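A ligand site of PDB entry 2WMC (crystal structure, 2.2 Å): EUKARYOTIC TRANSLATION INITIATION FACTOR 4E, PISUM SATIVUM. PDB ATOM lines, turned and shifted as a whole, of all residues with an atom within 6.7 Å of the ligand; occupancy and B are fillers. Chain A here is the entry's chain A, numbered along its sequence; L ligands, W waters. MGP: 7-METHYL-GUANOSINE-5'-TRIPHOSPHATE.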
ATOM      1  N   LYS A  19     -19.636  12.936  40.556  1.00  0.00           N
ATOM      2  CA  LYS A  19     -20.643  13.286  39.566  1.00  0.00           C
ATOM      3  C   LYS A  19     -21.541  14.305  40.222  1.00  0.00           C
ATOM      4  O   LYS A  19     -22.175  15.115  39.570  1.00  0.00           O
ATOM      5  CB  LYS A  19     -21.477  12.082  39.113  1.00  0.00           C
ATOM      6  CG  LYS A  19     -20.759  10.979  38.341  1.00  0.00           C
ATOM      7  CD  LYS A  19     -21.791  10.025  37.717  1.00  0.00           C
ATOM      8  CE  LYS A  19     -21.158   9.007  36.757  1.00  0.00           C
ATOM      9  NZ  LYS A  19     -21.990   7.759  36.491  1.00  0.00           N
ATOM     10  N   TRP A  25     -21.183  16.544  31.929  1.00  0.00           N
ATOM     11  CA  TRP A  25     -20.945  15.107  31.903  1.00  0.00           C
ATOM     12  C   TRP A  25     -19.444  14.811  31.792  1.00  0.00           C
ATOM     13  O   TRP A  25     -18.731  15.352  30.969  1.00  0.00           O
ATOM     14  CB  TRP A  25     -21.698  14.400  30.768  1.00  0.00           C
ATOM     15  CG  TRP A  25     -21.471  12.998  30.914  1.00  0.00           C
ATOM     16  CD1 TRP A  25     -22.189  12.137  31.677  1.00  0.00           C
ATOM     17  CD2 TRP A  25     -20.370  12.231  30.375  1.00  0.00           C
ATOM     18  NE1 TRP A  25     -21.637  10.880  31.631  1.00  0.00           N
ATOM     19  CE2 TRP A  25     -20.519  10.920  30.838  1.00  0.00           C
ATOM     20  CE3 TRP A  25     -19.299  12.545  29.537  1.00  0.00           C
ATOM     21  CZ2 TRP A  25     -19.626   9.909  30.482  1.00  0.00           C
ATOM     22  CZ3 TRP A  25     -18.426  11.532  29.192  1.00  0.00           C
ATOM     23  CH2 TRP A  25     -18.585  10.240  29.659  1.00  0.00           C
ATOM     24  N   GLY A  26     -18.998  13.930  32.686  1.00  0.00           N
ATOM     25  CA  GLY A  26     -17.674  13.309  32.628  1.00  0.00           C
ATOM     26  C   GLY A  26     -16.521  14.179  33.026  1.00  0.00           C
ATOM     27  O   GLY A  26     -15.365  13.765  32.919  1.00  0.00           O
ATOM     28  N   MET A  29     -14.558  12.649  35.821  1.00  0.00           N
ATOM     29  CA  MET A  29     -13.823  11.419  35.570  1.00  0.00           C
ATOM     30  C   MET A  29     -12.364  11.668  35.941  1.00  0.00           C
ATOM     31  O   MET A  29     -11.808  12.708  35.635  1.00  0.00           O
ATOM     32  CB  MET A  29     -13.967  11.075  34.079  1.00  0.00           C
ATOM     33  CG  MET A  29     -13.716   9.674  33.633  1.00  0.00           C
ATOM     34  SD  MET A  29     -13.765   9.784  31.827  1.00  0.00           S
ATOM     35  CE  MET A  29     -15.488   9.395  31.530  1.00  0.00           C
ATOM     36  N   ASP A  59     -19.006   4.523  37.292  1.00  0.00           N
ATOM     37  CA  ASP A  59     -18.443   4.046  36.030  1.00  0.00           C
ATOM     38  C   ASP A  59     -16.968   3.860  36.256  1.00  0.00           C
ATOM     39  O   ASP A  59     -16.293   4.715  36.850  1.00  0.00           O
ATOM     40  CB  ASP A  59     -18.659   5.042  34.894  1.00  0.00           C
ATOM     41  CG  ASP A  59     -20.129   5.353  34.649  1.00  0.00           C
ATOM     42  OD1 ASP A  59     -20.918   4.382  34.594  1.00  0.00           O
ATOM     43  OD2 ASP A  59     -20.464   6.561  34.495  1.00  0.00           O
ATOM     44  N   TYR A  61     -13.487   2.679  34.188  1.00  0.00           N
ATOM     45  CA  TYR A  61     -12.891   2.544  32.846  1.00  0.00           C
ATOM     46  C   TYR A  61     -11.489   1.990  32.835  1.00  0.00           C
ATOM     47  O   TYR A  61     -10.702   2.205  33.758  1.00  0.00           O
ATOM     48  CB  TYR A  61     -12.843   3.877  32.105  1.00  0.00           C
ATOM     49  CG  TYR A  61     -14.151   4.621  31.932  1.00  0.00           C
ATOM     50  CD1 TYR A  61     -14.669   5.406  32.942  1.00  0.00           C
ATOM     51  CD2 TYR A  61     -14.828   4.585  30.729  1.00  0.00           C
ATOM     52  CE1 TYR A  61     -15.831   6.110  32.788  1.00  0.00           C
ATOM     53  CE2 TYR A  61     -16.010   5.287  30.550  1.00  0.00           C
ATOM     54  CZ  TYR A  61     -16.503   6.055  31.591  1.00  0.00           C
ATOM     55  OH  TYR A  61     -17.664   6.760  31.437  1.00  0.00           O
ATOM     56  N   PRO A  69     -12.079   8.356  27.747  1.00  0.00           N
ATOM     57  CA  PRO A  69     -13.323   7.650  27.491  1.00  0.00           C
ATOM     58  C   PRO A  69     -14.469   8.577  27.231  1.00  0.00           C
ATOM     59  O   PRO A  69     -15.311   8.808  28.092  1.00  0.00           O
ATOM     60  CB  PRO A  69     -13.570   6.867  28.777  1.00  0.00           C
ATOM     61  CG  PRO A  69     -12.500   7.184  29.702  1.00  0.00           C
ATOM     62  CD  PRO A  69     -11.565   8.155  29.115  1.00  0.00           C
ATOM     63  N   LYS A  70     -14.482   9.076  25.999  1.00  0.00           N
ATOM     64  CA  LYS A  70     -15.440  10.083  25.569  1.00  0.00           C
ATOM     65  C   LYS A  70     -15.764  10.053  24.072  1.00  0.00           C
ATOM     66  O   LYS A  70     -14.894   9.909  23.223  1.00  0.00           O
ATOM     67  CB  LYS A  70     -14.937  11.465  25.950  1.00  0.00           C
ATOM     68  CG  LYS A  70     -15.420  11.866  27.322  1.00  0.00           C
ATOM     69  CD  LYS A  70     -14.494  12.895  27.976  1.00  0.00           C
ATOM     70  CE  LYS A  70     -14.712  12.889  29.468  1.00  0.00           C
ATOM     71  NZ  LYS A  70     -13.556  13.357  30.269  1.00  0.00           N
ATOM     72  N   TRP A  71     -17.050  10.217  23.808  1.00  0.00           N
ATOM     73  CA  TRP A  71     -17.566  10.287  22.438  1.00  0.00           C
ATOM     74  C   TRP A  71     -16.722  11.263  21.692  1.00  0.00           C
ATOM     75  O   TRP A  71     -16.324  11.032  20.550  1.00  0.00           O
ATOM     76  CB  TRP A  71     -19.010  10.787  22.413  1.00  0.00           C
ATOM     77  CG  TRP A  71     -19.883   9.795  23.057  1.00  0.00           C
ATOM     78  CD1 TRP A  71     -19.517   8.512  23.336  1.00  0.00           C
ATOM     79  CD2 TRP A  71     -21.229   9.945  23.530  1.00  0.00           C
ATOM     80  NE1 TRP A  71     -20.541   7.848  23.957  1.00  0.00           N
ATOM     81  CE2 TRP A  71     -21.609   8.702  24.085  1.00  0.00           C
ATOM     82  CE3 TRP A  71     -22.145  10.992  23.540  1.00  0.00           C
ATOM     83  CZ2 TRP A  71     -22.877   8.493  24.656  1.00  0.00           C
ATOM     84  CZ3 TRP A  71     -23.399  10.786  24.108  1.00  0.00           C
ATOM     85  CH2 TRP A  71     -23.751   9.535  24.645  1.00  0.00           C
ATOM     86  N   GLU A  72     -16.503  12.388  22.363  1.00  0.00           N
ATOM     87  CA  GLU A  72     -15.798  13.562  21.770  1.00  0.00           C
ATOM     88  C   GLU A  72     -14.273  13.499  21.849  1.00  0.00           C
ATOM     89  O   GLU A  72     -13.597  14.457  21.475  1.00  0.00           O
ATOM     90  CB  GLU A  72     -16.296  14.907  22.343  1.00  0.00           C
ATOM     91  CG  GLU A  72     -16.632  14.950  23.823  1.00  0.00           C
ATOM     92  CD  GLU A  72     -18.038  14.417  24.110  1.00  0.00           C
ATOM     93  OE1 GLU A  72     -18.988  14.809  23.399  1.00  0.00           O
ATOM     94  OE2 GLU A  72     -18.168  13.599  25.041  1.00  0.00           O
ATOM     95  N   LYS A  81     -19.531   1.186  20.446  1.00  0.00           N
ATOM     96  CA  LYS A  81     -19.436   0.276  21.589  1.00  0.00           C
ATOM     97  C   LYS A  81     -20.359  -0.920  21.487  1.00  0.00           C
ATOM     98  O   LYS A  81     -21.531  -0.806  21.122  1.00  0.00           O
ATOM     99  CB  LYS A  81     -19.702   1.011  22.898  1.00  0.00           C
ATOM    100  CG  LYS A  81     -21.108   1.576  23.026  1.00  0.00           C
ATOM    101  CD  LYS A  81     -21.371   1.983  24.427  1.00  0.00           C
ATOM    102  CE  LYS A  81     -22.795   2.500  24.597  1.00  0.00           C
ATOM    103  NZ  LYS A  81     -23.103   3.626  23.629  1.00  0.00           N
ATOM    104  N   ASN A 119     -20.436  -0.177  34.026  1.00  0.00           N
ATOM    105  CA  ASN A 119     -21.406   0.750  34.543  1.00  0.00           C
ATOM    106  C   ASN A 119     -22.238   0.077  35.588  1.00  0.00           C
ATOM    107  O   ASN A 119     -22.974  -0.863  35.287  1.00  0.00           O
ATOM    108  CB  ASN A 119     -22.329   1.198  33.433  1.00  0.00           C
ATOM    109  CG  ASN A 119     -21.606   1.779  32.248  1.00  0.00           C
ATOM    110  OD1 ASN A 119     -21.800   1.337  31.145  1.00  0.00           O
ATOM    111  ND2 ASN A 119     -20.814   2.820  32.469  1.00  0.00           N
ATOM    112  N   ARG A 121     -25.308   0.132  37.830  1.00  0.00           N
ATOM    113  CA  ARG A 121     -26.603   0.773  37.930  1.00  0.00           C
ATOM    114  C   ARG A 121     -27.545   0.066  38.891  1.00  0.00           C
ATOM    115  O   ARG A 121     -27.195  -0.895  39.557  1.00  0.00           O
ATOM    116  CB  ARG A 121     -27.257   0.841  36.577  1.00  0.00           C
ATOM    117  CG  ARG A 121     -26.412   1.589  35.558  1.00  0.00           C
ATOM    118  CD  ARG A 121     -26.218   3.048  35.988  1.00  0.00           C
ATOM    119  NE  ARG A 121     -25.461   3.838  35.015  1.00  0.00           N
ATOM    120  CZ  ARG A 121     -24.168   4.113  35.112  1.00  0.00           C
ATOM    121  NH1 ARG A 121     -23.461   3.662  36.123  1.00  0.00           N
ATOM    122  NH2 ARG A 121     -23.583   4.811  34.175  1.00  0.00           N
ATOM    123  N   LYS A 126     -23.612  -3.080  33.380  1.00  0.00           N
ATOM    124  CA  LYS A 126     -23.240  -3.163  31.952  1.00  0.00           C
ATOM    125  C   LYS A 126     -21.748  -3.143  31.783  1.00  0.00           C
ATOM    126  O   LYS A 126     -21.022  -2.437  32.486  1.00  0.00           O
ATOM    127  CB  LYS A 126     -23.760  -1.957  31.173  1.00  0.00           C
ATOM    128  CG  LYS A 126     -25.203  -1.608  31.416  1.00  0.00           C
ATOM    129  CD  LYS A 126     -25.722  -0.589  30.435  1.00  0.00           C
ATOM    130  CE  LYS A 126     -25.498   0.848  30.913  1.00  0.00           C
ATOM    131  NZ  LYS A 126     -25.881   1.873  29.854  1.00  0.00           N
ATOM    132  N   TRP A 130     -15.348  -0.220  23.890  1.00  0.00           N
ATOM    133  CA  TRP A 130     -15.315   0.929  23.009  1.00  0.00           C
ATOM    134  C   TRP A 130     -14.247   0.702  21.974  1.00  0.00           C
ATOM    135  O   TRP A 130     -13.086   0.405  22.310  1.00  0.00           O
ATOM    136  CB  TRP A 130     -14.969   2.193  23.779  1.00  0.00           C
ATOM    137  CG  TRP A 130     -16.050   2.802  24.540  1.00  0.00           C
ATOM    138  CD1 TRP A 130     -17.041   2.166  25.229  1.00  0.00           C
ATOM    139  CD2 TRP A 130     -16.240   4.203  24.736  1.00  0.00           C
ATOM    140  NE1 TRP A 130     -17.851   3.098  25.832  1.00  0.00           N
ATOM    141  CE2 TRP A 130     -17.377   4.355  25.536  1.00  0.00           C
ATOM    142  CE3 TRP A 130     -15.557   5.340  24.302  1.00  0.00           C
ATOM    143  CZ2 TRP A 130     -17.862   5.607  25.919  1.00  0.00           C
ATOM    144  CZ3 TRP A 130     -16.045   6.589  24.672  1.00  0.00           C
ATOM    145  CH2 TRP A 130     -17.183   6.705  25.461  1.00  0.00           C
ATOM    146  N   HIS A 162     -21.001   5.968  18.262  1.00  0.00           N
ATOM    147  CA  HIS A 162     -20.966   7.107  19.207  1.00  0.00           C
ATOM    148  C   HIS A 162     -21.706   8.304  18.619  1.00  0.00           C
ATOM    149  O   HIS A 162     -22.371   9.058  19.324  1.00  0.00           O
ATOM    150  CB  HIS A 162     -19.530   7.521  19.536  1.00  0.00           C
ATOM    151  CG  HIS A 162     -18.765   6.526  20.355  1.00  0.00           C
ATOM    152  ND1 HIS A 162     -19.348   5.751  21.324  1.00  0.00           N
ATOM    153  CD2 HIS A 162     -17.442   6.225  20.365  1.00  0.00           C
ATOM    154  CE1 HIS A 162     -18.420   4.987  21.883  1.00  0.00           C
ATOM    155  NE2 HIS A 162     -17.260   5.253  21.318  1.00  0.00           N
ATOM    156  N   ALA A 165     -24.962   8.226  19.285  1.00  0.00           N
ATOM    157  CA  ALA A 165     -25.158   8.357  20.744  1.00  0.00           C
ATOM    158  C   ALA A 165     -25.132   9.846  20.995  1.00  0.00           C
ATOM    159  O   ALA A 165     -25.919  10.381  21.770  1.00  0.00           O
ATOM    160  CB  ALA A 165     -24.043   7.636  21.536  1.00  0.00           C
ATOM    161  N   ARG A 166     -24.261  10.482  20.236  1.00  0.00           N
ATOM    162  CA  ARG A 166     -23.974  11.922  20.355  1.00  0.00           C
ATOM    163  C   ARG A 166     -25.174  12.758  19.908  1.00  0.00           C
ATOM    164  O   ARG A 166     -25.875  13.333  20.738  1.00  0.00           O
ATOM    165  CB  ARG A 166     -22.730  12.342  19.529  1.00  0.00           C
ATOM    166  CG  ARG A 166     -21.482  12.629  20.360  1.00  0.00           C
ATOM    167  CD  ARG A 166     -20.363  13.271  19.527  1.00  0.00           C
ATOM    168  NE  ARG A 166     -19.263  12.318  19.284  1.00  0.00           N
ATOM    169  CZ  ARG A 166     -19.157  11.567  18.195  1.00  0.00           C
ATOM    170  NH1 ARG A 166     -20.053  11.662  17.219  1.00  0.00           N
ATOM    171  NH2 ARG A 166     -18.139  10.710  18.068  1.00  0.00           N
ATOM    172  N   ARG A 170     -30.376   7.940  24.083  1.00  0.00           N
ATOM    173  CA  ARG A 170     -31.243   6.869  24.556  1.00  0.00           C
ATOM    174  C   ARG A 170     -32.139   6.431  23.408  1.00  0.00           C
ATOM    175  O   ARG A 170     -32.831   5.413  23.473  1.00  0.00           O
ATOM    176  CB  ARG A 170     -32.085   7.355  25.747  1.00  0.00           C
ATOM    177  CG  ARG A 170     -31.315   8.261  26.694  1.00  0.00           C
ATOM    178  CD  ARG A 170     -31.950   8.311  28.078  1.00  0.00           C
ATOM    179  NE  ARG A 170     -30.988   8.740  29.089  1.00  0.00           N
ATOM    180  CZ  ARG A 170     -30.287   7.873  29.817  1.00  0.00           C
ATOM    181  NH1 ARG A 170     -30.452   6.576  29.623  1.00  0.00           N
ATOM    182  NH2 ARG A 170     -29.420   8.304  30.738  1.00  0.00           N
HETATM  183  PA  MGP L   1     -25.569   6.632  31.363  1.00  0.00           P
HETATM  184  O1A MGP L   1     -25.806   7.234  32.703  1.00  0.00           O
HETATM  185  O2A MGP L   1     -24.427   5.692  31.123  1.00  0.00           O
HETATM  186  O3A MGP L   1     -26.976   5.943  30.872  1.00  0.00           O
HETATM  187  O5' MGP L   1     -25.428   7.848  30.307  1.00  0.00           O
HETATM  188  PB  MGP L   1     -27.738   5.041  31.912  1.00  0.00           P
HETATM  189  O1B MGP L   1     -29.321   5.095  31.672  1.00  0.00           O
HETATM  190  O2B MGP L   1     -27.542   5.823  33.303  1.00  0.00           O
HETATM  191  O3B MGP L   1     -27.263   3.631  31.937  1.00  0.00           O
HETATM  192  C5' MGP L   1     -26.260   8.924  30.602  1.00  0.00           C
HETATM  193  C4' MGP L   1     -25.931  10.130  29.736  1.00  0.00           C
HETATM  194  O4' MGP L   1     -24.566  10.447  30.025  1.00  0.00           O
HETATM  195  C3' MGP L   1     -25.928   9.828  28.245  1.00  0.00           C
HETATM  196  O3' MGP L   1     -27.265   9.838  27.716  1.00  0.00           O
HETATM  197  C2' MGP L   1     -25.233  11.103  27.831  1.00  0.00           C
HETATM  198  O2' MGP L   1     -26.116  12.198  28.053  1.00  0.00           O
HETATM  199  C1' MGP L   1     -24.123  11.196  28.876  1.00  0.00           C
HETATM  200  N9  MGP L   1     -22.949  10.605  28.275  1.00  0.00           N
HETATM  201  C8  MGP L   1     -22.519   9.345  28.340  1.00  0.00           C
HETATM  202  N7  MGP L   1     -21.376   9.279  27.647  1.00  0.00           N
HETATM  203  CM7 MGP L   1     -20.571   8.063  27.455  1.00  0.00           C
HETATM  204  C5  MGP L   1     -21.103  10.468  27.158  1.00  0.00           C
HETATM  205  C6  MGP L   1     -20.071  10.977  26.398  1.00  0.00           C
HETATM  206  O6  MGP L   1     -19.141  10.285  25.991  1.00  0.00           O
HETATM  207  N1  MGP L   1     -20.113  12.311  26.094  1.00  0.00           N
HETATM  208  C2  MGP L   1     -21.151  13.119  26.526  1.00  0.00           C
HETATM  209  N2  MGP L   1     -21.144  14.407  26.199  1.00  0.00           N
HETATM  210  N3  MGP L   1     -22.137  12.605  27.257  1.00  0.00           N
HETATM  211  C4  MGP L   1     -22.109  11.312  27.573  1.00  0.00           C
HETATM  212  O   HOH W   1     -29.148   2.495  33.540  1.00  0.00           O
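The backbone carbonyl oxygen (O) of Trp 71 lies within hydrogen-bond range of the guanidinium group (NH2) of Arg 166 (3.1 Å).
O of Gly 26 is in hydrogen-bond range of NZ of Lys 70, 3.2 Å away.
The guanidinium group (NH2) of Arg 121 is in salt-bridge range of the side-chain carboxylate (OD1) of Asp 59.
The backbone carbonyl oxygen of Lys 126 is in hydrogen-bond range of the backbone NH of Asn 119, at 2.8 Å.
The guanidinium group (NH1) of Arg 170 lies within salt-bridge range of an oxygen (O1B) of the ligand, 2.8 Å away.
An oxygen (O6) of the ligand lies close to the indole nitrogen (NE1) of Trp 71, at 3.5 Å.
An oxygen (O6) of the ligand is in hydrogen-bond range of the backbone NH (N) of Trp 71, at 3.0 Å.
The side-chain carboxylate (OE2) of Glu 72 lies within hydrogen-bond range of a nitrogen (N1) of the ligand, at 2.6 Å.
The indole nitrogen (NE1) of Trp 25 lies close to an oxygen (O4') of the ligand (3.4 Å).
The guanidinium group (NH2) of Arg 121 is in salt-bridge range of an oxygen (O2A) of the ligand, at 3.3 Å.
NZ of Lys 126 is in salt-bridge range of O3B of the ligand (3.1 Å).
Lys 70 touches the ligand (CA to O6, 3.7 Å).
Trp 130 touches the ligand.
Hydrophobic or aromatic side chains within 4 Å of the ligand: Trp 25, Trp 71 and Trp 130.
Along chain A the residues within 4 Å of the ligand span positions 25 to 170.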
